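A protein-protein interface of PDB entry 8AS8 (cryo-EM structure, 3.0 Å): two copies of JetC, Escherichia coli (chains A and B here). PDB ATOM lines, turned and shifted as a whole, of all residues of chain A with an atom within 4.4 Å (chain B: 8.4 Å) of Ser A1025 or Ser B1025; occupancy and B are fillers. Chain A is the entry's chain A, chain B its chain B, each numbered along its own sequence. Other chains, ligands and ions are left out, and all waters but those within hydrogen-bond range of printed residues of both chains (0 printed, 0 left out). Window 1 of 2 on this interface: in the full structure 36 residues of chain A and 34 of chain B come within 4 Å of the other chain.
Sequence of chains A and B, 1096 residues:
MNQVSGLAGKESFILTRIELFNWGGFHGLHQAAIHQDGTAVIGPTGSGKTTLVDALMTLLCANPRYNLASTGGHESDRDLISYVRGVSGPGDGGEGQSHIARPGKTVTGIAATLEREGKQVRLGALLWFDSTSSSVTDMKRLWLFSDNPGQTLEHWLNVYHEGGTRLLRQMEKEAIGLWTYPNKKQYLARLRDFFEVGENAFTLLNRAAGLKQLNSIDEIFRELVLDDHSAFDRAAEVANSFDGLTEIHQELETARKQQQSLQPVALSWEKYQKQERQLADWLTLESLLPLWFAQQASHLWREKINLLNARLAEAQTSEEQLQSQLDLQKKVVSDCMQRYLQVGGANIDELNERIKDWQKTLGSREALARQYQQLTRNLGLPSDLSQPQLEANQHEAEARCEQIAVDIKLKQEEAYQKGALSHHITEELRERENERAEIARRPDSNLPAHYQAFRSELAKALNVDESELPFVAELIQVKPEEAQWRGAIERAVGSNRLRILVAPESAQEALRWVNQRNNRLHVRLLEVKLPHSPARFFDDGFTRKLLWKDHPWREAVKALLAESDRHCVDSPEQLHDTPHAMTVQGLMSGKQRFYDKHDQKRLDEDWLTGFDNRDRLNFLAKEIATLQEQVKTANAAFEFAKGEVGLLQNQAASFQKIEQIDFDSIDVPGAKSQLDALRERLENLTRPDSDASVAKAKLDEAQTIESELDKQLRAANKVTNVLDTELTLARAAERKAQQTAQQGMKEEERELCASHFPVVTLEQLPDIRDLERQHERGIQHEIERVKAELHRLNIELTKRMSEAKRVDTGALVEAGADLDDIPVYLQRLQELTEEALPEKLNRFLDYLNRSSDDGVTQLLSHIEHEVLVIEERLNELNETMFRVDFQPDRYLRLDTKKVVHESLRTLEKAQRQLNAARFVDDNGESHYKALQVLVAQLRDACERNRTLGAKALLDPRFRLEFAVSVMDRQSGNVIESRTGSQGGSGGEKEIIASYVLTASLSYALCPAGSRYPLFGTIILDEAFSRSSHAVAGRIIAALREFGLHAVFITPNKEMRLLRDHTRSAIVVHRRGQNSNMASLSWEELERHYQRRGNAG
OG of Ser B1025 is in hydrogen-bond range of O of Ser A1025 (3.4 Å). NH2 of Arg A1026 sits at hydrogen-bond distance from O of Ala B69. The guanidinium group (NE) of Arg A1026 is in salt-bridge range of the side-chain carboxylate (OE2) of Glu B1022. NZ of Lys B1053 lies within hydrogen-bond range of O of Ser A1027. NZ of Lys A1053 lies within hydrogen-bond range of O of Phe B1024 (2.7 Å). NZ of Lys A1053 is in hydrogen-bond range of O of Ser B1027, at 3.2 Å. The side-chain amino group of Lys A1053 lies within salt-bridge range of the side-chain carboxylate of Glu B1054. The guanidinium group (NE) of Arg A1026 sits close to the side-chain amino group (NZ) of Lys B212, at 3.4 Å.
NZ of Lys A212 sits at hydrogen-bond distance from OG of Ser A1025. The side-chain amino group of Lys B212 lies within hydrogen-bond range of the backbone carbonyl oxygen of Ala B69 (2.6 Å). The backbone carbonyl oxygen (O) of Glu B1022 lies within hydrogen-bond range of the guanidinium group (NH1) of Arg B1026 (3.1 Å). The backbone NH (N) of Glu B1022 lies within hydrogen-bond range of the backbone carbonyl oxygen (O) of Ile B1049, 3.0 Å away. OG1 of Thr B1050 sits at hydrogen-bond distance from O of Lys B1053 (2.5 Å).
NZ of Lys B1053 touches O of Ser A1025, at 3.6 Å. Thr B45 touches Ser A1027 (OG1 to CA, 3.9 Å).
Of the printed residues of chain B, Ser A1025 touches Ser B1025 and Lys B1053. Printed residues of chain A within 4 Å of Phe B1024: Lys A1053 (2.7 Å). Of the printed residues of chain A, Ser B1027 touches Lys A1053 (3.2 Å). Of the printed residues of chain A, Lys B1053 touches Ser A1025 (3.6 Å) and Ser A1027 (2.9 Å). Of the printed residues of chain A, Glu B1054 touches Lys A1053. The nearest residue of chain B that does not touch Ser A1025 is Pro B1051 (4.9 Å). The nearest residue of chain A that does not touch Ser B1025 is Lys A1053 (4.2 Å).
Of the 9 printed residues of chain A, 4 touch a printed residue of chain B. Of the 19 printed residues of chain B, 9 touch a printed residue of chain A. Along chain B the printed residues that touch a printed residue of chain A span positions 45 to 1054.
Ser B1025 touches its own counterpart, Ser A1025. Ser A1025 touches Lys B1053, but with the chains exchanged Lys A1053 does not touch Ser B1025 (4.2 Å). Arg A1026 touches Lys B212, but with the chains exchanged Lys A212 does not touch Arg B1026 (4.7 Å). Ser A1027 touches Lys B1053, and with the chains exchanged Lys A1053 touches Ser B1027. Positions printed for both chains: 212, 990, 1022, 1023, 1024, 1025, 1026, 1027 and 1053.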
ATOM      1  N   LYS A 212     -18.727 -24.978 -21.261  1.00  0.00           N
ATOM      2  CA  LYS A 212     -17.575 -24.228 -21.757  1.00  0.00           C
ATOM      3  C   LYS A 212     -16.508 -25.157 -22.327  1.00  0.00           C
ATOM      4  O   LYS A 212     -16.039 -24.965 -23.455  1.00  0.00           O
ATOM      5  CB  LYS A 212     -16.990 -23.370 -20.636  1.00  0.00           C
ATOM      6  CG  LYS A 212     -17.495 -21.940 -20.618  1.00  0.00           C
ATOM      7  CD  LYS A 212     -16.725 -21.101 -19.614  1.00  0.00           C
ATOM      8  CE  LYS A 212     -15.404 -20.620 -20.189  1.00  0.00           C
ATOM      9  NZ  LYS A 212     -15.592 -19.546 -21.201  1.00  0.00           N
ATOM     10  N   GLU A 990     -18.816 -24.575 -31.411  1.00  0.00           N
ATOM     11  CA  GLU A 990     -19.660 -23.997 -30.375  1.00  0.00           C
ATOM     12  C   GLU A 990     -21.118 -23.962 -30.809  1.00  0.00           C
ATOM     13  O   GLU A 990     -22.014 -24.288 -30.025  1.00  0.00           O
ATOM     14  CB  GLU A 990     -19.170 -22.591 -30.035  1.00  0.00           C
ATOM     15  CG  GLU A 990     -20.182 -21.760 -29.283  1.00  0.00           C
ATOM     16  CD  GLU A 990     -19.780 -21.523 -27.846  1.00  0.00           C
ATOM     17  OE1 GLU A 990     -18.640 -21.881 -27.481  1.00  0.00           O
ATOM     18  OE2 GLU A 990     -20.605 -20.984 -27.080  1.00  0.00           O
ATOM     19  N   GLU A1022     -21.731 -18.830 -18.910  1.00  0.00           N
ATOM     20  CA  GLU A1022     -20.667 -18.414 -19.867  1.00  0.00           C
ATOM     21  C   GLU A1022     -20.713 -19.360 -21.064  1.00  0.00           C
ATOM     22  O   GLU A1022     -19.659 -19.929 -21.404  1.00  0.00           O
ATOM     23  CB  GLU A1022     -19.296 -18.420 -19.187  1.00  0.00           C
ATOM     24  CG  GLU A1022     -19.009 -17.153 -18.403  1.00  0.00           C
ATOM     25  CD  GLU A1022     -19.489 -17.174 -16.962  1.00  0.00           C
ATOM     26  OE1 GLU A1022     -19.110 -18.109 -16.229  1.00  0.00           O
ATOM     27  OE2 GLU A1022     -20.239 -16.255 -16.576  1.00  0.00           O
ATOM     28  N   ALA A1023     -21.884 -19.498 -21.690  1.00  0.00           N
ATOM     29  CA  ALA A1023     -22.030 -20.477 -22.760  1.00  0.00           C
ATOM     30  C   ALA A1023     -21.190 -20.115 -23.979  1.00  0.00           C
ATOM     31  O   ALA A1023     -20.433 -20.950 -24.488  1.00  0.00           O
ATOM     32  CB  ALA A1023     -23.501 -20.611 -23.149  1.00  0.00           C
ATOM     33  N   PHE A1024     -21.304 -18.883 -24.462  1.00  0.00           N
ATOM     34  CA  PHE A1024     -20.720 -18.482 -25.735  1.00  0.00           C
ATOM     35  C   PHE A1024     -19.453 -17.676 -25.491  1.00  0.00           C
ATOM     36  O   PHE A1024     -19.505 -16.591 -24.904  1.00  0.00           O
ATOM     37  CB  PHE A1024     -21.720 -17.671 -26.554  1.00  0.00           C
ATOM     38  CG  PHE A1024     -23.138 -18.083 -26.335  1.00  0.00           C
ATOM     39  CD1 PHE A1024     -23.568 -19.342 -26.711  1.00  0.00           C
ATOM     40  CD2 PHE A1024     -24.041 -17.222 -25.740  1.00  0.00           C
ATOM     41  CE1 PHE A1024     -24.870 -19.731 -26.504  1.00  0.00           C
ATOM     42  CE2 PHE A1024     -25.346 -17.606 -25.533  1.00  0.00           C
ATOM     43  CZ  PHE A1024     -25.760 -18.863 -25.915  1.00  0.00           C
ATOM     44  N   SER A1025     -18.321 -18.214 -25.935  1.00  0.00           N
ATOM     45  CA  SER A1025     -17.059 -17.484 -25.886  1.00  0.00           C
ATOM     46  C   SER A1025     -16.246 -17.571 -27.166  1.00  0.00           C
ATOM     47  O   SER A1025     -15.403 -16.697 -27.391  1.00  0.00           O
ATOM     48  CB  SER A1025     -16.199 -17.978 -24.720  1.00  0.00           C
ATOM     49  OG  SER A1025     -16.788 -17.640 -23.477  1.00  0.00           O
ATOM     50  N   ARG A1026     -16.458 -18.576 -28.011  1.00  0.00           N
ATOM     51  CA  ARG A1026     -15.673 -18.762 -29.222  1.00  0.00           C
ATOM     52  C   ARG A1026     -16.410 -18.328 -30.480  1.00  0.00           C
ATOM     53  O   ARG A1026     -15.837 -18.398 -31.570  1.00  0.00           O
ATOM     54  CB  ARG A1026     -15.258 -20.231 -29.353  1.00  0.00           C
ATOM     55  CG  ARG A1026     -14.830 -20.868 -28.045  1.00  0.00           C
ATOM     56  CD  ARG A1026     -13.321 -20.986 -27.951  1.00  0.00           C
ATOM     57  NE  ARG A1026     -12.826 -22.233 -28.522  1.00  0.00           N
ATOM     58  CZ  ARG A1026     -13.175 -23.442 -28.105  1.00  0.00           C
ATOM     59  NH1 ARG A1026     -14.024 -23.610 -27.106  1.00  0.00           N
ATOM     60  NH2 ARG A1026     -12.656 -24.509 -28.705  1.00  0.00           N
ATOM     61  N   SER A1027     -17.655 -17.882 -30.360  1.00  0.00           N
ATOM     62  CA  SER A1027     -18.483 -17.553 -31.506  1.00  0.00           C
ATOM     63  C   SER A1027     -18.687 -16.047 -31.602  1.00  0.00           C
ATOM     64  O   SER A1027     -18.684 -15.335 -30.596  1.00  0.00           O
ATOM     65  CB  SER A1027     -19.841 -18.252 -31.419  1.00  0.00           C
ATOM     66  OG  SER A1027     -20.389 -18.128 -30.119  1.00  0.00           O
ATOM     67  N   LYS A1053     -17.797  -9.355 -20.493  1.00  0.00           N
ATOM     68  CA  LYS A1053     -18.051  -9.357 -21.922  1.00  0.00           C
ATOM     69  C   LYS A1053     -19.501  -9.754 -22.183  1.00  0.00           C
ATOM     70  O   LYS A1053     -20.250 -10.122 -21.277  1.00  0.00           O
ATOM     71  CB  LYS A1053     -17.106 -10.322 -22.631  1.00  0.00           C
ATOM     72  CG  LYS A1053     -15.645 -10.157 -22.280  1.00  0.00           C
ATOM     73  CD  LYS A1053     -14.931 -11.493 -22.387  1.00  0.00           C
ATOM     74  CE  LYS A1053     -14.166 -11.619 -23.692  1.00  0.00           C
ATOM     75  NZ  LYS A1053     -12.708 -11.419 -23.491  1.00  0.00           N
ATOM     76  N   THR B  45     -17.291 -15.916 -37.581  1.00  0.00           N
ATOM     77  CA  THR B  45     -17.012 -17.377 -37.564  1.00  0.00           C
ATOM     78  C   THR B  45     -17.150 -17.921 -38.988  1.00  0.00           C
ATOM     79  O   THR B  45     -18.070 -17.471 -39.700  1.00  0.00           O
ATOM     80  CB  THR B  45     -17.937 -18.100 -36.576  1.00  0.00           C
ATOM     81  OG1 THR B  45     -17.451 -17.860 -35.255  1.00  0.00           O
ATOM     82  CG2 THR B  45     -18.028 -19.589 -36.826  1.00  0.00           C
ATOM     83  N   ALA B  69      -6.437 -24.027 -31.093  1.00  0.00           N
ATOM     84  CA  ALA B  69      -7.311 -23.249 -30.225  1.00  0.00           C
ATOM     85  C   ALA B  69      -8.715 -23.827 -30.134  1.00  0.00           C
ATOM     86  O   ALA B  69      -9.389 -23.623 -29.120  1.00  0.00           O
ATOM     87  CB  ALA B  69      -7.380 -21.801 -30.707  1.00  0.00           C
ATOM     88  N   LYS B 212      -4.703 -21.978 -24.338  1.00  0.00           N
ATOM     89  CA  LYS B 212      -5.913 -22.320 -23.598  1.00  0.00           C
ATOM     90  C   LYS B 212      -5.607 -23.159 -22.362  1.00  0.00           C
ATOM     91  O   LYS B 212      -4.455 -23.237 -21.923  1.00  0.00           O
ATOM     92  CB  LYS B 212      -6.895 -23.069 -24.501  1.00  0.00           C
ATOM     93  CG  LYS B 212      -8.350 -22.675 -24.304  1.00  0.00           C
ATOM     94  CD  LYS B 212      -8.647 -21.317 -24.917  1.00  0.00           C
ATOM     95  CE  LYS B 212      -8.703 -21.402 -26.433  1.00  0.00           C
ATOM     96  NZ  LYS B 212      -9.794 -22.304 -26.895  1.00  0.00           N
ATOM     97  N   GLU B 990      -4.345 -15.986 -12.834  1.00  0.00           N
ATOM     98  CA  GLU B 990      -4.206 -15.978 -14.285  1.00  0.00           C
ATOM     99  C   GLU B 990      -3.094 -15.035 -14.719  1.00  0.00           C
ATOM    100  O   GLU B 990      -2.338 -15.337 -15.649  1.00  0.00           O
ATOM    101  CB  GLU B 990      -5.529 -15.586 -14.938  1.00  0.00           C
ATOM    102  CG  GLU B 990      -5.608 -15.900 -16.422  1.00  0.00           C
ATOM    103  CD  GLU B 990      -6.971 -16.416 -16.838  1.00  0.00           C
ATOM    104  OE1 GLU B 990      -7.089 -16.950 -17.961  1.00  0.00           O
ATOM    105  OE2 GLU B 990      -7.926 -16.286 -16.043  1.00  0.00           O
ATOM    106  N   LEU B1020      -1.172 -15.966 -31.122  1.00  0.00           N
ATOM    107  CA  LEU B1020      -2.050 -16.658 -30.186  1.00  0.00           C
ATOM    108  C   LEU B1020      -3.477 -16.581 -30.701  1.00  0.00           C
ATOM    109  O   LEU B1020      -4.089 -15.511 -30.686  1.00  0.00           O
ATOM    110  CB  LEU B1020      -1.939 -16.064 -28.778  1.00  0.00           C
ATOM    111  CG  LEU B1020      -2.111 -14.559 -28.607  1.00  0.00           C
ATOM    112  CD1 LEU B1020      -3.524 -14.242 -28.169  1.00  0.00           C
ATOM    113  CD2 LEU B1020      -1.111 -14.029 -27.600  1.00  0.00           C
ATOM    114  N   ASP B1021      -3.991 -17.670 -31.286  1.00  0.00           N
ATOM    115  CA  ASP B1021      -5.374 -17.690 -31.845  1.00  0.00           C
ATOM    116  C   ASP B1021      -6.385 -17.592 -30.698  1.00  0.00           C
ATOM    117  O   ASP B1021      -6.028 -18.033 -29.588  1.00  0.00           O
ATOM    118  CB  ASP B1021      -5.609 -18.925 -32.720  1.00  0.00           C
ATOM    119  CG  ASP B1021      -6.481 -18.647 -33.932  1.00  0.00           C
ATOM    120  OD1 ASP B1021      -7.720 -18.693 -33.785  1.00  0.00           O
ATOM    121  OD2 ASP B1021      -5.917 -18.387 -35.013  1.00  0.00           O
ATOM    122  N   GLU B1022      -7.600 -17.085 -30.960  1.00  0.00           N
ATOM    123  CA  GLU B1022      -8.590 -16.854 -29.866  1.00  0.00           C
ATOM    124  C   GLU B1022      -7.839 -16.106 -28.769  1.00  0.00           C
ATOM    125  O   GLU B1022      -7.591 -16.720 -27.712  1.00  0.00           O
ATOM    126  CB  GLU B1022      -9.175 -18.179 -29.371  1.00  0.00           C
ATOM    127  CG  GLU B1022      -9.511 -19.144 -30.493  1.00  0.00           C
ATOM    128  CD  GLU B1022     -10.939 -19.661 -30.488  1.00  0.00           C
ATOM    129  OE1 GLU B1022     -11.845 -18.888 -30.122  1.00  0.00           O
ATOM    130  OE2 GLU B1022     -11.140 -20.837 -30.853  1.00  0.00           O
ATOM    131  N   ALA B1023      -7.540 -14.822 -28.988  1.00  0.00           N
ATOM    132  CA  ALA B1023      -6.661 -14.117 -28.063  1.00  0.00           C
ATOM    133  C   ALA B1023      -7.093 -14.251 -26.607  1.00  0.00           C
ATOM    134  O   ALA B1023      -6.376 -14.832 -25.786  1.00  0.00           O
ATOM    135  CB  ALA B1023      -6.584 -12.641 -28.460  1.00  0.00           C
ATOM    136  N   PHE B1024      -8.265 -13.720 -26.264  1.00  0.00           N
ATOM    137  CA  PHE B1024      -8.719 -13.713 -24.870  1.00  0.00           C
ATOM    138  C   PHE B1024     -10.225 -13.963 -24.852  1.00  0.00           C
ATOM    139  O   PHE B1024     -11.022 -13.024 -24.921  1.00  0.00           O
ATOM    140  CB  PHE B1024      -8.353 -12.405 -24.185  1.00  0.00           C
ATOM    141  CG  PHE B1024      -6.978 -11.911 -24.525  1.00  0.00           C
ATOM    142  CD1 PHE B1024      -5.864 -12.453 -23.911  1.00  0.00           C
ATOM    143  CD2 PHE B1024      -6.799 -10.914 -25.466  1.00  0.00           C
ATOM    144  CE1 PHE B1024      -4.598 -12.005 -24.226  1.00  0.00           C
ATOM    145  CE2 PHE B1024      -5.536 -10.462 -25.784  1.00  0.00           C
ATOM    146  CZ  PHE B1024      -4.434 -11.009 -25.163  1.00  0.00           C
ATOM    147  N   SER B1025     -10.601 -15.233 -24.747  1.00  0.00           N
ATOM    148  CA  SER B1025     -11.998 -15.618 -24.613  1.00  0.00           C
ATOM    149  C   SER B1025     -12.378 -15.953 -23.181  1.00  0.00           C
ATOM    150  O   SER B1025     -13.510 -15.683 -22.769  1.00  0.00           O
ATOM    151  CB  SER B1025     -12.303 -16.821 -25.509  1.00  0.00           C
ATOM    152  OG  SER B1025     -12.050 -16.520 -26.869  1.00  0.00           O
ATOM    153  N   ARG B1026     -11.453 -16.531 -22.421  1.00  0.00           N
ATOM    154  CA  ARG B1026     -11.667 -16.879 -21.026  1.00  0.00           C
ATOM    155  C   ARG B1026     -11.028 -15.881 -20.073  1.00  0.00           C
ATOM    156  O   ARG B1026     -10.957 -16.145 -18.870  1.00  0.00           O
ATOM    157  CB  ARG B1026     -11.125 -18.282 -20.753  1.00  0.00           C
ATOM    158  CG  ARG B1026      -9.620 -18.402 -20.939  1.00  0.00           C
ATOM    159  CD  ARG B1026      -9.250 -18.523 -22.411  1.00  0.00           C
ATOM    160  NE  ARG B1026      -7.809 -18.452 -22.623  1.00  0.00           N
ATOM    161  CZ  ARG B1026      -7.237 -18.142 -23.778  1.00  0.00           C
ATOM    162  NH1 ARG B1026      -7.956 -17.872 -24.855  1.00  0.00           N
ATOM    163  NH2 ARG B1026      -5.911 -18.101 -23.855  1.00  0.00           N
ATOM    164  N   SER B1027     -10.562 -14.743 -20.580  1.00  0.00           N
ATOM    165  CA  SER B1027      -9.850 -13.756 -19.782  1.00  0.00           C
ATOM    166  C   SER B1027     -10.615 -12.442 -19.777  1.00  0.00           C
ATOM    167  O   SER B1027     -11.103 -11.992 -20.818  1.00  0.00           O
ATOM    168  CB  SER B1027      -8.434 -13.534 -20.318  1.00  0.00           C
ATOM    169  OG  SER B1027      -7.835 -14.761 -20.693  1.00  0.00           O
ATOM    170  N   SER B1028     -10.711 -11.830 -18.600  1.00  0.00           N
ATOM    171  CA  SER B1028     -11.404 -10.561 -18.466  1.00  0.00           C
ATOM    172  C   SER B1028     -10.582  -9.435 -19.090  1.00  0.00           C
ATOM    173  O   SER B1028      -9.380  -9.562 -19.336  1.00  0.00           O
ATOM    174  CB  SER B1028     -11.684 -10.257 -16.997  1.00  0.00           C
ATOM    175  OG  SER B1028     -10.546  -9.691 -16.372  1.00  0.00           O
ATOM    176  N   ALA B1032      -6.496  -9.181 -19.563  1.00  0.00           N
ATOM    177  CA  ALA B1032      -5.954  -9.241 -20.917  1.00  0.00           C
ATOM    178  C   ALA B1032      -4.994  -8.089 -21.176  1.00  0.00           C
ATOM    179  O   ALA B1032      -3.951  -8.269 -21.819  1.00  0.00           O
ATOM    180  CB  ALA B1032      -7.090  -9.235 -21.938  1.00  0.00           C
ATOM    181  N   ILE B1049      -5.589 -12.918 -32.583  1.00  0.00           N
ATOM    182  CA  ILE B1049      -6.746 -13.324 -33.436  1.00  0.00           C
ATOM    183  C   ILE B1049      -8.007 -13.384 -32.570  1.00  0.00           C
ATOM    184  O   ILE B1049      -8.023 -14.187 -31.629  1.00  0.00           O
ATOM    185  CB  ILE B1049      -6.468 -14.677 -34.123  1.00  0.00           C
ATOM    186  CG1 ILE B1049      -5.202 -14.629 -34.982  1.00  0.00           C
ATOM    187  CG2 ILE B1049      -7.676 -15.135 -34.925  1.00  0.00           C
ATOM    188  CD1 ILE B1049      -5.406 -15.119 -36.396  1.00  0.00           C
ATOM    189  N   THR B1050      -9.027 -12.588 -32.892  1.00  0.00           N
ATOM    190  CA  THR B1050     -10.268 -12.527 -32.141  1.00  0.00           C
ATOM    191  C   THR B1050     -11.437 -12.625 -33.105  1.00  0.00           C
ATOM    192  O   THR B1050     -11.317 -12.238 -34.272  1.00  0.00           O
ATOM    193  CB  THR B1050     -10.376 -11.230 -31.327  1.00  0.00           C
ATOM    194  OG1 THR B1050     -11.693 -11.117 -30.776  1.00  0.00           O
ATOM    195  CG2 THR B1050     -10.101 -10.031 -32.210  1.00  0.00           C
ATOM    196  N   PRO B1051     -12.573 -13.141 -32.650  1.00  0.00           N
ATOM    197  CA  PRO B1051     -13.773 -13.196 -33.499  1.00  0.00           C
ATOM    198  C   PRO B1051     -14.577 -11.898 -33.430  1.00  0.00           C
ATOM    199  O   PRO B1051     -15.750 -11.880 -33.052  1.00  0.00           O
ATOM    200  CB  PRO B1051     -14.531 -14.389 -32.909  1.00  0.00           C
ATOM    201  CG  PRO B1051     -14.191 -14.348 -31.461  1.00  0.00           C
ATOM    202  CD  PRO B1051     -12.800 -13.767 -31.338  1.00  0.00           C
ATOM    203  N   LYS B1053     -14.141  -9.642 -31.321  1.00  0.00           N
ATOM    204  CA  LYS B1053     -14.420  -9.460 -29.907  1.00  0.00           C
ATOM    205  C   LYS B1053     -13.239  -8.791 -29.221  1.00  0.00           C
ATOM    206  O   LYS B1053     -12.084  -8.971 -29.617  1.00  0.00           O
ATOM    207  CB  LYS B1053     -14.724 -10.797 -29.223  1.00  0.00           C
ATOM    208  CG  LYS B1053     -16.188 -11.182 -29.251  1.00  0.00           C
ATOM    209  CD  LYS B1053     -16.365 -12.686 -29.205  1.00  0.00           C
ATOM    210  CE  LYS B1053     -16.888 -13.133 -27.855  1.00  0.00           C
ATOM    211  NZ  LYS B1053     -17.940 -14.175 -27.990  1.00  0.00           N
ATOM    212  N   GLU B1054     -13.543  -8.019 -28.180  1.00  0.00           N
ATOM    213  CA  GLU B1054     -12.530  -7.308 -27.409  1.00  0.00           C
ATOM    214  C   GLU B1054     -11.797  -6.295 -28.287  1.00  0.00           C
ATOM    215  O   GLU B1054     -10.569  -6.267 -28.369  1.00  0.00           O
ATOM    216  CB  GLU B1054     -11.551  -8.290 -26.762  1.00  0.00           C
ATOM    217  CG  GLU B1054     -11.219  -7.950 -25.329  1.00  0.00           C
ATOM    218  CD  GLU B1054     -11.073  -9.176 -24.457  1.00  0.00           C
ATOM    219  OE1 GLU B1054     -10.214 -10.027 -24.766  1.00  0.00           O
ATOM    220  OE2 GLU B1054     -11.819  -9.291 -23.462  1.00  0.00           O
